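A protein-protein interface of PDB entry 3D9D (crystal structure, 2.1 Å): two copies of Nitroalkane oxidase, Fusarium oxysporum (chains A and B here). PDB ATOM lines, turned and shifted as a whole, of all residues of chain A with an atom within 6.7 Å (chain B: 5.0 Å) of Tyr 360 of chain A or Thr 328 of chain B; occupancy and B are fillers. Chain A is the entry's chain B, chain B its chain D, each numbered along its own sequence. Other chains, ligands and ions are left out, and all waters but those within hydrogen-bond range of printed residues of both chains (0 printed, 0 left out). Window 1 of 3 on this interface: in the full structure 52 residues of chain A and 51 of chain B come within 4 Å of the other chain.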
ATOM      1  N   ILE A 324      -4.872 -11.748 -29.346  1.00  0.00           N
ATOM      2  CA  ILE A 324      -5.935 -11.989 -28.375  1.00  0.00           C
ATOM      3  C   ILE A 324      -6.880 -13.124 -28.844  1.00  0.00           C
ATOM      4  O   ILE A 324      -7.319 -13.953 -28.026  1.00  0.00           O
ATOM      5  CB  ILE A 324      -6.739 -10.703 -28.154  1.00  0.00           C
ATOM      6  CG1 ILE A 324      -5.880  -9.635 -27.410  1.00  0.00           C
ATOM      7  CG2 ILE A 324      -8.079 -11.005 -27.464  1.00  0.00           C
ATOM      8  CD1 ILE A 324      -6.579  -8.242 -27.304  1.00  0.00           C
ATOM      9  N   ARG A 325      -7.181 -13.154 -30.154  1.00  0.00           N
ATOM     10  CA  ARG A 325      -8.013 -14.217 -30.725  1.00  0.00           C
ATOM     11  C   ARG A 325      -7.327 -15.579 -30.567  1.00  0.00           C
ATOM     12  O   ARG A 325      -7.967 -16.534 -30.155  1.00  0.00           O
ATOM     13  CB  ARG A 325      -8.330 -13.965 -32.192  1.00  0.00           C
ATOM     14  CG  ARG A 325      -9.381 -12.868 -32.424  1.00  0.00           C
ATOM     15  CD  ARG A 325      -9.444 -12.604 -33.910  1.00  0.00           C
ATOM     16  NE  ARG A 325     -10.238 -11.425 -34.273  1.00  0.00           N
ATOM     17  CZ  ARG A 325      -9.760 -10.413 -35.012  1.00  0.00           C
ATOM     18  NH1 ARG A 325      -8.468 -10.405 -35.466  1.00  0.00           N
ATOM     19  NH2 ARG A 325     -10.582  -9.403 -35.303  1.00  0.00           N
ATOM     20  N   LEU A 326      -6.029 -15.634 -30.867  1.00  0.00           N
ATOM     21  CA  LEU A 326      -5.229 -16.853 -30.733  1.00  0.00           C
ATOM     22  C   LEU A 326      -5.102 -17.294 -29.276  1.00  0.00           C
ATOM     23  O   LEU A 326      -5.238 -18.479 -28.949  1.00  0.00           O
ATOM     24  CB  LEU A 326      -3.837 -16.656 -31.361  1.00  0.00           C
ATOM     25  CG  LEU A 326      -3.840 -16.662 -32.896  1.00  0.00           C
ATOM     26  CD1 LEU A 326      -2.587 -15.992 -33.470  1.00  0.00           C
ATOM     27  CD2 LEU A 326      -3.977 -18.122 -33.448  1.00  0.00           C
ATOM     28  N   GLU A 327      -4.837 -16.329 -28.400  1.00  0.00           N
ATOM     29  CA  GLU A 327      -4.594 -16.637 -27.006  1.00  0.00           C
ATOM     30  C   GLU A 327      -5.865 -17.169 -26.348  1.00  0.00           C
ATOM     31  O   GLU A 327      -5.828 -18.163 -25.634  1.00  0.00           O
ATOM     32  CB  GLU A 327      -4.145 -15.377 -26.265  1.00  0.00           C
ATOM     33  CG  GLU A 327      -3.299 -15.656 -25.076  1.00  0.00           C
ATOM     34  CD  GLU A 327      -1.825 -15.832 -25.460  1.00  0.00           C
ATOM     35  OE1 GLU A 327      -1.133 -14.823 -25.804  1.00  0.00           O
ATOM     36  OE2 GLU A 327      -1.384 -16.990 -25.410  1.00  0.00           O
ATOM     37  N   THR A 328      -6.978 -16.456 -26.548  1.00  0.00           N
ATOM     38  CA  THR A 328      -8.256 -16.872 -25.999  1.00  0.00           C
ATOM     39  C   THR A 328      -8.691 -18.214 -26.592  1.00  0.00           C
ATOM     40  O   THR A 328      -9.237 -19.048 -25.871  1.00  0.00           O
ATOM     41  CB  THR A 328      -9.355 -15.827 -26.180  1.00  0.00           C
ATOM     42  OG1 THR A 328      -9.451 -15.468 -27.571  1.00  0.00           O
ATOM     43  CG2 THR A 328      -9.052 -14.573 -25.292  1.00  0.00           C
ATOM     44  N   SER A 329      -8.419 -18.425 -27.887  1.00  0.00           N
ATOM     45  CA  SER A 329      -8.682 -19.733 -28.530  1.00  0.00           C
ATOM     46  C   SER A 329      -7.993 -20.922 -27.843  1.00  0.00           C
ATOM     47  O   SER A 329      -8.692 -21.870 -27.429  1.00  0.00           O
ATOM     48  CB  SER A 329      -8.371 -19.703 -30.039  1.00  0.00           C
ATOM     49  OG  SER A 329      -9.310 -18.871 -30.736  1.00  0.00           O
ATOM     50  N   ARG A 330      -6.656 -20.892 -27.736  1.00  0.00           N
ATOM     51  CA  ARG A 330      -5.882 -22.020 -27.113  1.00  0.00           C
ATOM     52  C   ARG A 330      -6.367 -22.288 -25.694  1.00  0.00           C
ATOM     53  O   ARG A 330      -6.542 -23.415 -25.314  1.00  0.00           O
ATOM     54  CB  ARG A 330      -4.373 -21.764 -27.075  1.00  0.00           C
ATOM     55  CG  ARG A 330      -3.488 -23.031 -26.834  1.00  0.00           C
ATOM     56  CD  ARG A 330      -2.038 -22.845 -27.404  1.00  0.00           C
ATOM     57  NE  ARG A 330      -1.712 -21.499 -27.098  1.00  0.00           N
ATOM     58  CZ  ARG A 330      -1.217 -20.551 -27.871  1.00  0.00           C
ATOM     59  NH1 ARG A 330      -0.792 -20.739 -29.108  1.00  0.00           N
ATOM     60  NH2 ARG A 330      -1.098 -19.392 -27.296  1.00  0.00           N
ATOM     61  N   LEU A 331      -6.580 -21.223 -24.924  1.00  0.00           N
ATOM     62  CA  LEU A 331      -7.114 -21.350 -23.582  1.00  0.00           C
ATOM     63  C   LEU A 331      -8.435 -22.140 -23.576  1.00  0.00           C
ATOM     64  O   LEU A 331      -8.597 -23.083 -22.770  1.00  0.00           O
ATOM     65  CB  LEU A 331      -7.302 -19.961 -22.999  1.00  0.00           C
ATOM     66  CG  LEU A 331      -6.308 -19.315 -22.014  1.00  0.00           C
ATOM     67  CD1 LEU A 331      -4.949 -19.950 -21.979  1.00  0.00           C
ATOM     68  CD2 LEU A 331      -6.211 -17.799 -22.119  1.00  0.00           C
ATOM     69  N   LEU A 332      -9.356 -21.778 -24.481  1.00  0.00           N
ATOM     70  CA  LEU A 332     -10.675 -22.424 -24.582  1.00  0.00           C
ATOM     71  C   LEU A 332     -10.572 -23.889 -24.995  1.00  0.00           C
ATOM     72  O   LEU A 332     -11.235 -24.733 -24.411  1.00  0.00           O
ATOM     73  CB  LEU A 332     -11.604 -21.657 -25.554  1.00  0.00           C
ATOM     74  CG  LEU A 332     -13.079 -22.029 -25.604  1.00  0.00           C
ATOM     75  CD1 LEU A 332     -13.710 -21.992 -24.185  1.00  0.00           C
ATOM     76  CD2 LEU A 332     -13.871 -21.117 -26.549  1.00  0.00           C
ATOM     77  N   MET A 355     -19.003 -27.396 -27.700  1.00  0.00           N
ATOM     78  CA  MET A 355     -19.723 -26.562 -28.681  1.00  0.00           C
ATOM     79  C   MET A 355     -19.197 -25.115 -28.690  1.00  0.00           C
ATOM     80  O   MET A 355     -18.815 -24.589 -29.755  1.00  0.00           O
ATOM     81  CB  MET A 355     -21.244 -26.615 -28.420  1.00  0.00           C
ATOM     82  CG  MET A 355     -21.944 -27.996 -28.652  1.00  0.00           C
ATOM     83  SD  MET A 355     -21.524 -28.982 -30.124  1.00  0.00           S
ATOM     84  CE  MET A 355     -20.172 -29.925 -29.461  1.00  0.00           C
ATOM     85  N   GLN A 356     -19.147 -24.495 -27.507  1.00  0.00           N
ATOM     86  CA  GLN A 356     -18.493 -23.197 -27.302  1.00  0.00           C
ATOM     87  C   GLN A 356     -17.196 -23.142 -28.062  1.00  0.00           C
ATOM     88  O   GLN A 356     -16.942 -22.213 -28.846  1.00  0.00           O
ATOM     89  CB  GLN A 356     -18.094 -22.986 -25.815  1.00  0.00           C
ATOM     90  CG  GLN A 356     -19.216 -22.678 -24.913  1.00  0.00           C
ATOM     91  CD  GLN A 356     -18.770 -22.152 -23.601  1.00  0.00           C
ATOM     92  OE1 GLN A 356     -18.878 -22.815 -22.585  1.00  0.00           O
ATOM     93  NE2 GLN A 356     -18.260 -20.950 -23.601  1.00  0.00           N
ATOM     94  N   THR A 357     -16.346 -24.121 -27.754  1.00  0.00           N
ATOM     95  CA  THR A 357     -14.992 -24.185 -28.278  1.00  0.00           C
ATOM     96  C   THR A 357     -14.958 -24.179 -29.786  1.00  0.00           C
ATOM     97  O   THR A 357     -14.270 -23.347 -30.374  1.00  0.00           O
ATOM     98  CB  THR A 357     -14.244 -25.391 -27.721  1.00  0.00           C
ATOM     99  OG1 THR A 357     -14.295 -25.312 -26.294  1.00  0.00           O
ATOM    100  CG2 THR A 357     -12.768 -25.377 -28.180  1.00  0.00           C
ATOM    101  N   LYS A 358     -15.728 -25.083 -30.406  1.00  0.00           N
ATOM    102  CA  LYS A 358     -15.749 -25.191 -31.858  1.00  0.00           C
ATOM    103  C   LYS A 358     -16.220 -23.868 -32.506  1.00  0.00           C
ATOM    104  O   LYS A 358     -15.613 -23.401 -33.471  1.00  0.00           O
ATOM    105  CB  LYS A 358     -16.657 -26.372 -32.271  1.00  0.00           C
ATOM    106  CG  LYS A 358     -16.304 -27.101 -33.569  1.00  0.00           C
ATOM    107  CD  LYS A 358     -16.402 -26.187 -34.788  1.00  0.00           C
ATOM    108  CE  LYS A 358     -16.732 -26.968 -36.068  1.00  0.00           C
ATOM    109  NZ  LYS A 358     -17.291 -26.064 -37.150  1.00  0.00           N
ATOM    110  N   ILE A 359     -17.298 -23.276 -31.985  1.00  0.00           N
ATOM    111  CA  ILE A 359     -17.891 -22.067 -32.568  1.00  0.00           C
ATOM    112  C   ILE A 359     -16.896 -20.868 -32.512  1.00  0.00           C
ATOM    113  O   ILE A 359     -16.618 -20.214 -33.523  1.00  0.00           O
ATOM    114  CB  ILE A 359     -19.214 -21.697 -31.855  1.00  0.00           C
ATOM    115  CG1 ILE A 359     -20.294 -22.789 -32.043  1.00  0.00           C
ATOM    116  CG2 ILE A 359     -19.727 -20.354 -32.321  1.00  0.00           C
ATOM    117  CD1 ILE A 359     -21.383 -22.748 -31.002  1.00  0.00           C
ATOM    118  N   TYR A 360     -16.344 -20.627 -31.327  1.00  0.00           N
ATOM    119  CA  TYR A 360     -15.495 -19.482 -31.096  1.00  0.00           C
ATOM    120  C   TYR A 360     -14.229 -19.602 -31.912  1.00  0.00           C
ATOM    121  O   TYR A 360     -13.924 -18.717 -32.715  1.00  0.00           O
ATOM    122  CB  TYR A 360     -15.140 -19.335 -29.609  1.00  0.00           C
ATOM    123  CG  TYR A 360     -14.224 -18.140 -29.361  1.00  0.00           C
ATOM    124  CD1 TYR A 360     -14.722 -16.841 -29.410  1.00  0.00           C
ATOM    125  CD2 TYR A 360     -12.863 -18.310 -29.128  1.00  0.00           C
ATOM    126  CE1 TYR A 360     -13.893 -15.728 -29.200  1.00  0.00           C
ATOM    127  CE2 TYR A 360     -12.023 -17.208 -28.897  1.00  0.00           C
ATOM    128  CZ  TYR A 360     -12.555 -15.923 -28.949  1.00  0.00           C
ATOM    129  OH  TYR A 360     -11.732 -14.839 -28.765  1.00  0.00           O
ATOM    130  N   THR A 361     -13.500 -20.710 -31.711  1.00  0.00           N
ATOM    131  CA  THR A 361     -12.176 -20.848 -32.271  1.00  0.00           C
ATOM    132  C   THR A 361     -12.223 -20.762 -33.801  1.00  0.00           C
ATOM    133  O   THR A 361     -11.311 -20.188 -34.434  1.00  0.00           O
ATOM    134  CB  THR A 361     -11.467 -22.167 -31.876  1.00  0.00           C
ATOM    135  OG1 THR A 361     -12.292 -23.304 -32.201  1.00  0.00           O
ATOM    136  CG2 THR A 361     -11.086 -22.195 -30.399  1.00  0.00           C
ATOM    137  N   THR A 362     -13.272 -21.336 -34.392  1.00  0.00           N
ATOM    138  CA  THR A 362     -13.315 -21.413 -35.838  1.00  0.00           C
ATOM    139  C   THR A 362     -13.735 -20.090 -36.471  1.00  0.00           C
ATOM    140  O   THR A 362     -13.197 -19.702 -37.523  1.00  0.00           O
ATOM    141  CB  THR A 362     -14.188 -22.579 -36.362  1.00  0.00           C
ATOM    142  OG1 THR A 362     -15.550 -22.422 -35.945  1.00  0.00           O
ATOM    143  CG2 THR A 362     -13.633 -23.934 -35.876  1.00  0.00           C
ATOM    144  N   ASP A 363     -14.687 -19.404 -35.842  1.00  0.00           N
ATOM    145  CA  ASP A 363     -15.154 -18.126 -36.341  1.00  0.00           C
ATOM    146  C   ASP A 363     -14.005 -17.105 -36.244  1.00  0.00           C
ATOM    147  O   ASP A 363     -13.778 -16.336 -37.183  1.00  0.00           O
ATOM    148  CB  ASP A 363     -16.383 -17.627 -35.545  1.00  0.00           C
ATOM    149  CG  ASP A 363     -17.716 -18.292 -35.988  1.00  0.00           C
ATOM    150  OD1 ASP A 363     -18.715 -18.178 -35.228  1.00  0.00           O
ATOM    151  OD2 ASP A 363     -17.765 -18.905 -37.081  1.00  0.00           O
ATOM    152  N   VAL A 364     -13.296 -17.083 -35.115  1.00  0.00           N
ATOM    153  CA  VAL A 364     -12.282 -16.047 -34.915  1.00  0.00           C
ATOM    154  C   VAL A 364     -10.983 -16.333 -35.632  1.00  0.00           C
ATOM    155  O   VAL A 364     -10.227 -15.409 -35.907  1.00  0.00           O
ATOM    156  CB  VAL A 364     -12.058 -15.611 -33.438  1.00  0.00           C
ATOM    157  CG1 VAL A 364     -13.384 -15.370 -32.736  1.00  0.00           C
ATOM    158  CG2 VAL A 364     -11.188 -16.632 -32.662  1.00  0.00           C
ATOM    159  N   ALA A 365     -10.710 -17.604 -35.952  1.00  0.00           N
ATOM    160  CA  ALA A 365      -9.500 -17.906 -36.722  1.00  0.00           C
ATOM    161  C   ALA A 365      -9.583 -17.272 -38.118  1.00  0.00           C
ATOM    162  O   ALA A 365      -8.593 -16.744 -38.604  1.00  0.00           O
ATOM    163  CB  ALA A 365      -9.238 -19.429 -36.818  1.00  0.00           C
ATOM    164  N   ASN A 404     -21.026 -24.290 -37.632  1.00  0.00           N
ATOM    165  CA  ASN A 404     -21.489 -23.540 -36.510  1.00  0.00           C
ATOM    166  C   ASN A 404     -22.955 -23.189 -36.592  1.00  0.00           C
ATOM    167  O   ASN A 404     -23.661 -23.201 -35.551  1.00  0.00           O
ATOM    168  CB  ASN A 404     -20.639 -22.282 -36.358  1.00  0.00           C
ATOM    169  CG  ASN A 404     -19.191 -22.616 -36.179  1.00  0.00           C
ATOM    170  OD1 ASN A 404     -18.835 -23.785 -35.962  1.00  0.00           O
ATOM    171  ND2 ASN A 404     -18.332 -21.601 -36.248  1.00  0.00           N
ATOM    172  N   ILE B 324     -19.941 -17.501 -24.525  1.00  0.00           N
ATOM    173  CA  ILE B 324     -18.603 -17.626 -25.068  1.00  0.00           C
ATOM    174  C   ILE B 324     -17.669 -16.467 -24.629  1.00  0.00           C
ATOM    175  O   ILE B 324     -16.533 -16.705 -24.224  1.00  0.00           O
ATOM    176  CB  ILE B 324     -18.708 -17.674 -26.606  1.00  0.00           C
ATOM    177  CG1 ILE B 324     -19.259 -19.043 -27.042  1.00  0.00           C
ATOM    178  CG2 ILE B 324     -17.376 -17.369 -27.261  1.00  0.00           C
ATOM    179  CD1 ILE B 324     -19.468 -19.184 -28.545  1.00  0.00           C
ATOM    180  N   ARG B 325     -18.157 -15.231 -24.703  1.00  0.00           N
ATOM    181  CA  ARG B 325     -17.417 -14.063 -24.217  1.00  0.00           C
ATOM    182  C   ARG B 325     -17.042 -14.158 -22.721  1.00  0.00           C
ATOM    183  O   ARG B 325     -15.957 -13.777 -22.323  1.00  0.00           O
ATOM    184  CB  ARG B 325     -18.226 -12.781 -24.488  1.00  0.00           C
ATOM    185  CG  ARG B 325     -18.251 -12.394 -25.989  1.00  0.00           C
ATOM    186  CD  ARG B 325     -19.095 -11.159 -26.178  1.00  0.00           C
ATOM    187  NE  ARG B 325     -19.370 -10.888 -27.585  1.00  0.00           N
ATOM    188  CZ  ARG B 325     -20.586 -10.908 -28.127  1.00  0.00           C
ATOM    189  NH1 ARG B 325     -20.684 -10.647 -29.420  1.00  0.00           N
ATOM    190  NH2 ARG B 325     -21.705 -11.186 -27.386  1.00  0.00           N
ATOM    191  N   LEU B 326     -17.948 -14.674 -21.914  1.00  0.00           N
ATOM    192  CA  LEU B 326     -17.684 -14.814 -20.498  1.00  0.00           C
ATOM    193  C   LEU B 326     -16.650 -15.932 -20.238  1.00  0.00           C
ATOM    194  O   LEU B 326     -15.754 -15.778 -19.383  1.00  0.00           O
ATOM    195  CB  LEU B 326     -18.975 -15.125 -19.764  1.00  0.00           C
ATOM    196  CG  LEU B 326     -19.928 -13.935 -19.684  1.00  0.00           C
ATOM    197  CD1 LEU B 326     -21.357 -14.401 -19.415  1.00  0.00           C
ATOM    198  CD2 LEU B 326     -19.464 -12.976 -18.647  1.00  0.00           C
ATOM    199  N   GLU B 327     -16.748 -17.019 -20.994  1.00  0.00           N
ATOM    200  CA  GLU B 327     -15.889 -18.160 -20.767  1.00  0.00           C
ATOM    201  C   GLU B 327     -14.422 -17.865 -21.137  1.00  0.00           C
ATOM    202  O   GLU B 327     -13.521 -18.101 -20.318  1.00  0.00           O
ATOM    203  CB  GLU B 327     -16.384 -19.353 -21.535  1.00  0.00           C
ATOM    204  CG  GLU B 327     -15.637 -20.616 -21.188  1.00  0.00           C
ATOM    205  CD  GLU B 327     -15.773 -20.983 -19.701  1.00  0.00           C
ATOM    206  OE1 GLU B 327     -16.929 -21.071 -19.198  1.00  0.00           O
ATOM    207  OE2 GLU B 327     -14.708 -21.154 -19.039  1.00  0.00           O
ATOM    208  N   THR B 328     -14.215 -17.385 -22.365  1.00  0.00           N
ATOM    209  CA  THR B 328     -12.928 -16.900 -22.831  1.00  0.00           C
ATOM    210  C   THR B 328     -12.357 -15.782 -21.934  1.00  0.00           C
ATOM    211  O   THR B 328     -11.187 -15.829 -21.622  1.00  0.00           O
ATOM    212  CB  THR B 328     -12.976 -16.455 -24.319  1.00  0.00           C
ATOM    213  OG1 THR B 328     -13.902 -15.372 -24.473  1.00  0.00           O
ATOM    214  CG2 THR B 328     -13.385 -17.623 -25.239  1.00  0.00           C
ATOM    215  N   SER B 329     -13.174 -14.823 -21.484  1.00  0.00           N
ATOM    216  CA  SER B 329     -12.691 -13.795 -20.556  1.00  0.00           C
ATOM    217  C   SER B 329     -12.156 -14.371 -19.243  1.00  0.00           C
ATOM    218  O   SER B 329     -11.078 -13.989 -18.807  1.00  0.00           O
ATOM    219  CB  SER B 329     -13.756 -12.739 -20.223  1.00  0.00           C
ATOM    220  OG  SER B 329     -14.242 -12.070 -21.365  1.00  0.00           O
ATOM    221  N   ARG B 330     -12.920 -15.247 -18.596  1.00  0.00           N
ATOM    222  CA  ARG B 330     -12.463 -15.850 -17.331  1.00  0.00           C
ATOM    223  C   ARG B 330     -11.165 -16.642 -17.504  1.00  0.00           C
ATOM    224  O   ARG B 330     -10.227 -16.483 -16.741  1.00  0.00           O
ATOM    225  CB  ARG B 330     -13.541 -16.736 -16.686  1.00  0.00           C
ATOM    226  CG  ARG B 330     -13.175 -17.097 -15.253  1.00  0.00           C
ATOM    227  CD  ARG B 330     -14.119 -18.100 -14.647  1.00  0.00           C
ATOM    228  NE  ARG B 330     -15.441 -17.510 -14.480  1.00  0.00           N
ATOM    229  CZ  ARG B 330     -16.492 -17.823 -15.232  1.00  0.00           C
ATOM    230  NH1 ARG B 330     -16.360 -18.719 -16.186  1.00  0.00           N
ATOM    231  NH2 ARG B 330     -17.672 -17.240 -15.011  1.00  0.00           N
ATOM    232  N   LEU B 331     -11.114 -17.494 -18.505  1.00  0.00           N
ATOM    233  CA  LEU B 331      -9.889 -18.238 -18.815  1.00  0.00           C
ATOM    234  C   LEU B 331      -8.644 -17.304 -18.977  1.00  0.00           C
ATOM    235  O   LEU B 331      -7.532 -17.601 -18.472  1.00  0.00           O
ATOM    236  CB  LEU B 331     -10.124 -19.026 -20.101  1.00  0.00           C
ATOM    237  CG  LEU B 331     -10.443 -20.531 -20.154  1.00  0.00           C
ATOM    238  CD1 LEU B 331     -10.787 -21.197 -18.846  1.00  0.00           C
ATOM    239  CD2 LEU B 331     -11.433 -20.905 -21.282  1.00  0.00           C
ATOM    240  N   LEU B 332      -8.848 -16.212 -19.707  1.00  0.00           N
ATOM    241  CA  LEU B 332      -7.797 -15.220 -19.949  1.00  0.00           C
ATOM    242  C   LEU B 332      -7.358 -14.524 -18.661  1.00  0.00           C
ATOM    243  O   LEU B 332      -6.173 -14.358 -18.435  1.00  0.00           O
ATOM    244  CB  LEU B 332      -8.272 -14.176 -20.957  1.00  0.00           C
ATOM    245  CG  LEU B 332      -7.243 -13.199 -21.556  1.00  0.00           C
ATOM    246  CD1 LEU B 332      -5.962 -13.895 -22.107  1.00  0.00           C
ATOM    247  CD2 LEU B 332      -7.917 -12.325 -22.635  1.00  0.00           C
ATOM    248  N   TYR B 360      -9.308  -7.311 -24.066  1.00  0.00           N
ATOM    249  CA  TYR B 360     -10.321  -8.302 -24.443  1.00  0.00           C
ATOM    250  C   TYR B 360     -11.497  -8.310 -23.490  1.00  0.00           C
ATOM    251  O   TYR B 360     -12.640  -8.115 -23.916  1.00  0.00           O
ATOM    252  CB  TYR B 360      -9.737  -9.721 -24.536  1.00  0.00           C
ATOM    253  CG  TYR B 360     -10.796 -10.745 -24.967  1.00  0.00           C
ATOM    254  CD1 TYR B 360     -11.218 -10.799 -26.290  1.00  0.00           C
ATOM    255  CD2 TYR B 360     -11.398 -11.622 -24.045  1.00  0.00           C
ATOM    256  CE1 TYR B 360     -12.166 -11.708 -26.702  1.00  0.00           C
ATOM    257  CE2 TYR B 360     -12.388 -12.558 -24.462  1.00  0.00           C
ATOM    258  CZ  TYR B 360     -12.754 -12.572 -25.805  1.00  0.00           C
ATOM    259  OH  TYR B 360     -13.698 -13.425 -26.299  1.00  0.00           O
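The side-chain hydroxyl (OH) of Tyr 360 of chain A sits at hydrogen-bond distance from the side-chain hydroxyl (OH) of Tyr 360 of chain B (3.5 Å).
The backbone carbonyl oxygen of Arg 325 of chain A is in hydrogen-bond range of the side-chain hydroxyl of Thr 328 of chain A (3.2 Å). The backbone carbonyl oxygen of Ile 359 of chain A lies within hydrogen-bond range of the side-chain hydroxyl of Thr 362 of chain A, 3.4 Å away. NH1 of Arg 330 of chain B is in salt-bridge range of OE1 of Glu 327 of chain B, 3.9 Å away. The side-chain hydroxyl (OH) of Tyr 360 of chain A is in hydrogen-bond range of the side-chain hydroxyl (OG1) of Thr 328 of chain A (2.7 Å). The backbone carbonyl oxygen (O) of Ile 324 of chain A is in hydrogen-bond range of the side-chain hydroxyl (OG1) of Thr 328 of chain A, 2.7 Å away. The backbone carbonyl oxygen (O) of Ile 324 of chain B lies within hydrogen-bond range of the side-chain hydroxyl (OG1) of Thr 328 of chain B, 3.0 Å away.
Among the printed residues, merely in contact across the chains: Ile 324 of chain A with Tyr 360 of chain B, Thr 328 of chain A with Leu 332 of chain B, Thr 328 of chain A with Tyr 360 of chain B, Leu 331 of chain A with Leu 331 of chain B, Leu 331 of chain A with Leu 332 of chain B, Leu 332 of chain A with Glu 327 of chain B, Leu 332 of chain A with Thr 328 of chain B, Leu 332 of chain A with Leu 331 of chain B, Gln 356 of chain A with Ile 324 of chain B, Gln 356 of chain A with Glu 327 of chain B, Ile 359 of chain A with Ile 324 of chain B, Tyr 360 of chain A with Ile 324 of chain B and Tyr 360 of chain A with Thr 328 of chain B.
Leu 326 of chain A touches none of the printed residues of chain B. Of the printed residues of chain B, Thr 328 of chain A touches Leu 332 and Tyr 360. Printed residues of chain A within 4 Å of Ile 324 of chain B: Gln 356, Ile 359 and Tyr 360. Of chain A, only Leu 332 and Tyr 360 come within 4 Å of Thr 328 of chain B. Ser 329 of chain B touches none of the printed residues of chain A. The nearest printed residue of chain B that does not touch Tyr 360 of chain A is Arg 325 of chain B (6.0 Å). The nearest residue of chain A that does not touch Thr 328 of chain B is Thr 328 of chain A (4.1 Å). The nearest printed residue of chain A that does not touch Glu 327 of chain B is Leu 331 of chain A (7.0 Å).
Of the 21 printed residues of chain A, 7 touch a printed residue of chain B. Hydrophobic or aromatic side chains of chain A within 4 Å of the printed part of chain B: Ile 324, Leu 331, Leu 332, Ile 359 and Tyr 360. Printed residues of chain B that touch a printed residue of chain A: Ile 324, Glu 327, Thr 328, Leu 331, Leu 332 and Tyr 360. Hydrophobic or aromatic side chains of chain B that line the printed part of chain A: Ile 324, Leu 331, Leu 332 and Tyr 360. Among the printed residues, 14 pairs touch across the chains.
Thr 328 of chain A touches Leu 332 of chain B, and with the chains exchanged Leu 332 of chain A touches Thr 328 of chain B. Leu 331 of chain A touches its own counterpart, Leu 331 of chain B. Leu 331 of chain A touches Leu 332 of chain B, and with the chains exchanged Leu 332 of chain A touches Leu 331 of chain B. Tyr 360 of chain A touches its own counterpart, Tyr 360 of chain B. Of the 14 pairs that touch across the chains among the printed residues, 10 have their exchanged pair printed and touching as well.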
